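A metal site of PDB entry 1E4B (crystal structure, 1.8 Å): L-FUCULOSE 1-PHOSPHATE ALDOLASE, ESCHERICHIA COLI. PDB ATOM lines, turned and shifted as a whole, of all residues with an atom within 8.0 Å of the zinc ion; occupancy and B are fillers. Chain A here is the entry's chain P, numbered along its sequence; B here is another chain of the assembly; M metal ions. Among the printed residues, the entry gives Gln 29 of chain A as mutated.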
ATOM      1  N   THR A  26      12.025  16.477  25.198  1.00  0.00           N
ATOM      2  CA  THR A  26      12.504  17.797  24.776  1.00  0.00           C
ATOM      3  C   THR A  26      14.011  17.832  24.575  1.00  0.00           C
ATOM      4  O   THR A  26      14.629  18.888  24.702  1.00  0.00           O
ATOM      5  CB  THR A  26      12.125  18.832  25.863  1.00  0.00           C
ATOM      6  OG1 THR A  26      12.869  18.564  27.061  1.00  0.00           O
ATOM      7  CG2 THR A  26      10.631  18.790  26.159  1.00  0.00           C
ATOM      8  N   ALA A  27      14.607  16.681  24.291  1.00  0.00           N
ATOM      9  CA  ALA A  27      16.056  16.587  24.202  1.00  0.00           C
ATOM     10  C   ALA A  27      16.700  17.278  23.010  1.00  0.00           C
ATOM     11  O   ALA A  27      17.747  17.920  23.173  1.00  0.00           O
ATOM     12  CB  ALA A  27      16.438  15.108  24.230  1.00  0.00           C
ATOM     13  N   GLY A  28      16.159  17.181  21.802  1.00  0.00           N
ATOM     14  CA  GLY A  28      16.832  17.781  20.667  1.00  0.00           C
ATOM     15  C   GLY A  28      16.568  19.253  20.417  1.00  0.00           C
ATOM     16  O   GLY A  28      15.684  19.892  20.959  1.00  0.00           O
ATOM     17  N   GLN A  29      17.349  19.817  19.484  1.00  0.00           N
ATOM     18  CA  GLN A  29      17.210  21.163  19.007  1.00  0.00           C
ATOM     19  C   GLN A  29      17.710  21.171  17.546  1.00  0.00           C
ATOM     20  O   GLN A  29      18.566  20.386  17.216  1.00  0.00           O
ATOM     21  CB  GLN A  29      18.066  22.268  19.589  1.00  0.00           C
ATOM     22  CG  GLN A  29      18.173  22.464  21.050  1.00  0.00           C
ATOM     23  CD  GLN A  29      19.315  21.642  21.610  1.00  0.00           C
ATOM     24  OE1 GLN A  29      20.382  21.553  20.988  1.00  0.00           O
ATOM     25  NE2 GLN A  29      19.000  21.116  22.777  1.00  0.00           N
ATOM     26  N   SER A  71      17.139  27.656  23.386  1.00  0.00           N
ATOM     27  CA  SER A  71      17.489  26.365  23.967  1.00  0.00           C
ATOM     28  C   SER A  71      18.625  26.569  24.953  1.00  0.00           C
ATOM     29  O   SER A  71      19.561  27.340  24.704  1.00  0.00           O
ATOM     30  CB  SER A  71      18.059  25.469  22.844  1.00  0.00           C
ATOM     31  OG  SER A  71      18.680  24.339  23.409  1.00  0.00           O
ATOM     32  N   SER A  72      18.666  25.755  25.999  1.00  0.00           N
ATOM     33  CA  SER A  72      19.734  25.789  26.990  1.00  0.00           C
ATOM     34  C   SER A  72      21.066  25.369  26.378  1.00  0.00           C
ATOM     35  O   SER A  72      22.116  25.715  26.917  1.00  0.00           O
ATOM     36  CB  SER A  72      19.379  24.860  28.157  1.00  0.00           C
ATOM     37  OG  SER A  72      19.203  23.529  27.670  1.00  0.00           O
ATOM     38  N   GLU A  73      21.034  24.683  25.239  1.00  0.00           N
ATOM     39  CA  GLU A  73      22.247  24.231  24.571  1.00  0.00           C
ATOM     40  C   GLU A  73      22.553  25.068  23.339  1.00  0.00           C
ATOM     41  O   GLU A  73      23.226  24.574  22.428  1.00  0.00           O
ATOM     42  CB  GLU A  73      22.081  22.745  24.184  1.00  0.00           C
ATOM     43  CG  GLU A  73      21.478  21.870  25.273  1.00  0.00           C
ATOM     44  CD  GLU A  73      21.954  20.421  25.173  1.00  0.00           C
ATOM     45  OE1 GLU A  73      23.155  20.178  25.402  1.00  0.00           O
ATOM     46  OE2 GLU A  73      21.138  19.528  24.876  1.00  0.00           O
ATOM     47  N   PHE A  76      26.710  25.679  21.733  1.00  0.00           N
ATOM     48  CA  PHE A  76      27.506  24.842  20.818  1.00  0.00           C
ATOM     49  C   PHE A  76      26.955  24.866  19.393  1.00  0.00           C
ATOM     50  O   PHE A  76      27.654  24.442  18.462  1.00  0.00           O
ATOM     51  CB  PHE A  76      27.782  23.459  21.357  1.00  0.00           C
ATOM     52  CG  PHE A  76      26.694  22.479  21.655  1.00  0.00           C
ATOM     53  CD1 PHE A  76      25.549  22.372  20.883  1.00  0.00           C
ATOM     54  CD2 PHE A  76      26.837  21.648  22.758  1.00  0.00           C
ATOM     55  CE1 PHE A  76      24.584  21.435  21.217  1.00  0.00           C
ATOM     56  CE2 PHE A  76      25.864  20.717  23.088  1.00  0.00           C
ATOM     57  CZ  PHE A  76      24.728  20.617  22.307  1.00  0.00           C
ATOM     58  N   HIS A  77      25.750  25.399  19.171  1.00  0.00           N
ATOM     59  CA  HIS A  77      25.227  25.607  17.812  1.00  0.00           C
ATOM     60  C   HIS A  77      26.015  26.774  17.222  1.00  0.00           C
ATOM     61  O   HIS A  77      26.570  26.688  16.123  1.00  0.00           O
ATOM     62  CB  HIS A  77      23.735  25.941  17.821  1.00  0.00           C
ATOM     63  CG  HIS A  77      22.864  24.757  18.149  1.00  0.00           C
ATOM     64  ND1 HIS A  77      22.070  24.166  17.179  1.00  0.00           N
ATOM     65  CD2 HIS A  77      22.694  24.050  19.290  1.00  0.00           C
ATOM     66  CE1 HIS A  77      21.416  23.138  17.721  1.00  0.00           C
ATOM     67  NE2 HIS A  77      21.771  23.054  19.005  1.00  0.00           N
ATOM     68  N   HIS A  92      21.014  18.661  16.876  1.00  0.00           N
ATOM     69  CA  HIS A  92      21.555  18.013  18.068  1.00  0.00           C
ATOM     70  C   HIS A  92      20.446  17.119  18.642  1.00  0.00           C
ATOM     71  O   HIS A  92      19.286  17.505  18.686  1.00  0.00           O
ATOM     72  CB  HIS A  92      21.998  19.044  19.108  1.00  0.00           C
ATOM     73  CG  HIS A  92      22.294  18.480  20.460  1.00  0.00           C
ATOM     74  ND1 HIS A  92      23.261  17.537  20.710  1.00  0.00           N
ATOM     75  CD2 HIS A  92      21.702  18.749  21.652  1.00  0.00           C
ATOM     76  CE1 HIS A  92      23.277  17.261  22.007  1.00  0.00           C
ATOM     77  NE2 HIS A  92      22.335  17.985  22.591  1.00  0.00           N
ATOM     78  N   ASN A  93      20.791  15.942  19.141  1.00  0.00           N
ATOM     79  CA  ASN A  93      19.800  15.113  19.789  1.00  0.00           C
ATOM     80  C   ASN A  93      20.546  14.182  20.731  1.00  0.00           C
ATOM     81  O   ASN A  93      21.779  14.171  20.770  1.00  0.00           O
ATOM     82  CB  ASN A  93      18.950  14.298  18.835  1.00  0.00           C
ATOM     83  CG  ASN A  93      19.751  13.377  17.932  1.00  0.00           C
ATOM     84  OD1 ASN A  93      20.651  12.680  18.364  1.00  0.00           O
ATOM     85  ND2 ASN A  93      19.408  13.409  16.638  1.00  0.00           N
ATOM     86  N   HIS A  94      19.757  13.459  21.484  1.00  0.00           N
ATOM     87  CA  HIS A  94      20.310  12.466  22.407  1.00  0.00           C
ATOM     88  C   HIS A  94      19.816  11.100  21.955  1.00  0.00           C
ATOM     89  O   HIS A  94      19.385  10.318  22.788  1.00  0.00           O
ATOM     90  CB  HIS A  94      19.937  12.757  23.851  1.00  0.00           C
ATOM     91  CG  HIS A  94      20.270  14.082  24.448  1.00  0.00           C
ATOM     92  ND1 HIS A  94      19.945  14.384  25.759  1.00  0.00           N
ATOM     93  CD2 HIS A  94      20.946  15.170  23.985  1.00  0.00           C
ATOM     94  CE1 HIS A  94      20.352  15.633  26.036  1.00  0.00           C
ATOM     95  NE2 HIS A  94      20.967  16.111  24.947  1.00  0.00           N
ATOM     96  N   PHE A 131      26.908  20.640  30.096  1.00  0.00           N
ATOM     97  CA  PHE A 131      26.092  21.196  29.040  1.00  0.00           C
ATOM     98  C   PHE A 131      26.016  22.716  29.190  1.00  0.00           C
ATOM     99  O   PHE A 131      26.038  23.248  30.312  1.00  0.00           O
ATOM    100  CB  PHE A 131      24.657  20.637  29.043  1.00  0.00           C
ATOM    101  CG  PHE A 131      23.718  21.099  30.119  1.00  0.00           C
ATOM    102  CD1 PHE A 131      23.728  20.510  31.376  1.00  0.00           C
ATOM    103  CD2 PHE A 131      22.803  22.116  29.881  1.00  0.00           C
ATOM    104  CE1 PHE A 131      22.861  20.918  32.369  1.00  0.00           C
ATOM    105  CE2 PHE A 131      21.942  22.543  30.886  1.00  0.00           C
ATOM    106  CZ  PHE A 131      21.950  21.943  32.132  1.00  0.00           C
ATOM    107  N   GLY A 132      25.955  23.402  28.053  1.00  0.00           N
ATOM    108  CA  GLY A 132      25.815  24.836  28.045  1.00  0.00           C
ATOM    109  C   GLY A 132      27.043  25.646  28.383  1.00  0.00           C
ATOM    110  O   GLY A 132      26.938  26.876  28.491  1.00  0.00           O
ATOM    111  N   LEU A 136      32.548  22.993  26.767  1.00  0.00           N
ATOM    112  CA  LEU A 136      31.878  22.061  25.870  1.00  0.00           C
ATOM    113  C   LEU A 136      31.898  22.597  24.436  1.00  0.00           C
ATOM    114  O   LEU A 136      32.136  21.866  23.492  1.00  0.00           O
ATOM    115  CB  LEU A 136      30.402  21.876  26.234  1.00  0.00           C
ATOM    116  CG  LEU A 136      29.757  20.504  26.080  1.00  0.00           C
ATOM    117  CD1 LEU A 136      28.251  20.574  25.843  1.00  0.00           C
ATOM    118  CD2 LEU A 136      30.471  19.568  25.131  1.00  0.00           C
ATOM    119  N   LEU A 152      29.147  13.274  21.605  1.00  0.00           N
ATOM    120  CA  LEU A 152      29.522  14.101  22.762  1.00  0.00           C
ATOM    121  C   LEU A 152      29.513  13.105  23.941  1.00  0.00           C
ATOM    122  O   LEU A 152      28.451  12.542  24.188  1.00  0.00           O
ATOM    123  CB  LEU A 152      28.477  15.185  22.996  1.00  0.00           C
ATOM    124  CG  LEU A 152      28.473  16.413  22.077  1.00  0.00           C
ATOM    125  CD1 LEU A 152      27.997  16.047  20.689  1.00  0.00           C
ATOM    126  CD2 LEU A 152      27.525  17.464  22.640  1.00  0.00           C
ATOM    127  N   HIS A 154      28.991  10.978  27.153  1.00  0.00           N
ATOM    128  CA  HIS A 154      27.933  11.010  28.146  1.00  0.00           C
ATOM    129  C   HIS A 154      26.800  11.986  27.810  1.00  0.00           C
ATOM    130  O   HIS A 154      26.170  12.560  28.708  1.00  0.00           O
ATOM    131  CB  HIS A 154      28.451  11.374  29.551  1.00  0.00           C
ATOM    132  CG  HIS A 154      29.292  10.322  30.177  1.00  0.00           C
ATOM    133  ND1 HIS A 154      28.802   9.106  30.647  1.00  0.00           N
ATOM    134  CD2 HIS A 154      30.623  10.311  30.454  1.00  0.00           C
ATOM    135  CE1 HIS A 154      29.818   8.407  31.150  1.00  0.00           C
ATOM    136  NE2 HIS A 154      30.928   9.111  31.058  1.00  0.00           N
ATOM    137  N   HIS A 155      26.494  12.126  26.496  1.00  0.00           N
ATOM    138  CA  HIS A 155      25.547  13.185  26.142  1.00  0.00           C
ATOM    139  C   HIS A 155      24.761  12.908  24.875  1.00  0.00           C
ATOM    140  O   HIS A 155      23.550  12.759  25.029  1.00  0.00           O
ATOM    141  CB  HIS A 155      26.323  14.512  26.029  1.00  0.00           C
ATOM    142  CG  HIS A 155      25.481  15.728  25.808  1.00  0.00           C
ATOM    143  ND1 HIS A 155      25.841  16.955  26.309  1.00  0.00           N
ATOM    144  CD2 HIS A 155      24.286  15.918  25.196  1.00  0.00           C
ATOM    145  CE1 HIS A 155      24.904  17.819  26.004  1.00  0.00           C
ATOM    146  NE2 HIS A 155      23.956  17.251  25.295  1.00  0.00           N
ATOM    147  N   GLY A 156      25.382  12.887  23.697  1.00  0.00           N
ATOM    148  CA  GLY A 156      24.540  12.715  22.492  1.00  0.00           C
ATOM    149  C   GLY A 156      25.319  12.996  21.212  1.00  0.00           C
ATOM    150  O   GLY A 156      26.494  12.653  21.115  1.00  0.00           O
ATOM    151  N   LEU A 157      24.651  13.631  20.263  1.00  0.00           N
ATOM    152  CA  LEU A 157      25.223  13.837  18.927  1.00  0.00           C
ATOM    153  C   LEU A 157      24.982  15.244  18.422  1.00  0.00           C
ATOM    154  O   LEU A 157      23.916  15.819  18.688  1.00  0.00           O
ATOM    155  CB  LEU A 157      24.417  12.854  18.035  1.00  0.00           C
ATOM    156  CG  LEU A 157      24.533  12.735  16.526  1.00  0.00           C
ATOM    157  CD1 LEU A 157      23.895  13.892  15.798  1.00  0.00           C
ATOM    158  CD2 LEU A 157      25.953  12.577  16.006  1.00  0.00           C
ATOM    159  N   HIS B 112      24.683   9.191  32.314  1.00  0.00           N
ATOM    160  CA  HIS B 112      24.252  10.291  31.483  1.00  0.00           C
ATOM    161  C   HIS B 112      23.819  11.457  32.378  1.00  0.00           C
ATOM    162  O   HIS B 112      23.318  11.166  33.493  1.00  0.00           O
ATOM    163  CB  HIS B 112      23.083   9.867  30.575  1.00  0.00           C
ATOM    164  CG  HIS B 112      22.819  10.823  29.461  1.00  0.00           C
ATOM    165  ND1 HIS B 112      22.077  11.963  29.641  1.00  0.00           N
ATOM    166  CD2 HIS B 112      23.195  10.791  28.149  1.00  0.00           C
ATOM    167  CE1 HIS B 112      22.034  12.628  28.492  1.00  0.00           C
ATOM    168  NE2 HIS B 112      22.687  11.939  27.585  1.00  0.00           N
ATOM    169  N   TYR B 113      24.012  12.697  31.923  1.00  0.00           N
ATOM    170  CA  TYR B 113      23.686  13.817  32.803  1.00  0.00           C
ATOM    171  C   TYR B 113      22.218  13.993  33.082  1.00  0.00           C
ATOM    172  O   TYR B 113      21.893  14.552  34.143  1.00  0.00           O
ATOM    173  CB  TYR B 113      24.345  15.140  32.380  1.00  0.00           C
ATOM    174  CG  TYR B 113      23.683  15.795  31.213  1.00  0.00           C
ATOM    175  CD1 TYR B 113      24.089  15.482  29.905  1.00  0.00           C
ATOM    176  CD2 TYR B 113      22.650  16.698  31.355  1.00  0.00           C
ATOM    177  CE1 TYR B 113      23.491  16.058  28.818  1.00  0.00           C
ATOM    178  CE2 TYR B 113      22.046  17.302  30.262  1.00  0.00           C
ATOM    179  CZ  TYR B 113      22.477  16.981  28.998  1.00  0.00           C
ATOM    180  OH  TYR B 113      21.876  17.571  27.908  1.00  0.00           O
ATOM    181  N   MET B 114      21.316  13.457  32.268  1.00  0.00           N
ATOM    182  CA  MET B 114      19.894  13.556  32.489  1.00  0.00           C
ATOM    183  C   MET B 114      19.416  12.695  33.651  1.00  0.00           C
ATOM    184  O   MET B 114      18.306  12.938  34.137  1.00  0.00           O
ATOM    185  CB  MET B 114      19.079  13.238  31.226  1.00  0.00           C
ATOM    186  CG  MET B 114      19.255  14.388  30.207  1.00  0.00           C
ATOM    187  SD  MET B 114      18.427  15.887  30.797  1.00  0.00           S
ATOM    188  CE  MET B 114      16.737  15.301  30.870  1.00  0.00           C
HETATM  189 ZN    ZN M   1      22.060  17.803  24.616  1.00  0.00          ZN
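O of Gln 29 sits at hydrogen-bond distance from N of His 92 (3.0 Å). The backbone NH (N) of Glu 73 lies within hydrogen-bond range of the side-chain hydroxyl (OG) of Ser 71, at 3.0 Å. A ring nitrogen (NE2) of His 94 lies close to the side-chain hydroxyl (OH) of Tyr 113 of chain B, 3.4 Å away. A ring nitrogen (ND1) of His 92 sits at hydrogen-bond distance from the backbone carbonyl oxygen (O) of Leu 157, at 2.7 Å. OE2 of Glu 73 lies close to NE2 of Gln 29 (3.4 Å). O of His 155 lies within hydrogen-bond range of NE2 of His 112 of chain B. The side-chain hydroxyl (OH) of Tyr 113 of chain B sits close to a ring nitrogen (NE2) of His 155 (3.4 Å).
The zinc ion is bound by the side-chain carboxylate (OE2) of Glu 73 (2.0 Å). A ring nitrogen (NE2) of His 94 is bound to the zinc ion (2.0 Å). NE2 of His 92 is bound to the zinc ion, 2.1 Å away. NE2 of His 155 binds the zinc ion, 2.1 Å away. The zinc ion has four donor atoms within binding distance. Slightly farther from the zinc ion lies the side-chain carboxylate (OE1) of Glu 73 (2.7 Å).
Tyr 113 of chain B touches the zinc ion. Within 4 Å of the zinc ion: Glu 73, His 92, His 94, His 155 and Tyr 113 of chain B.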
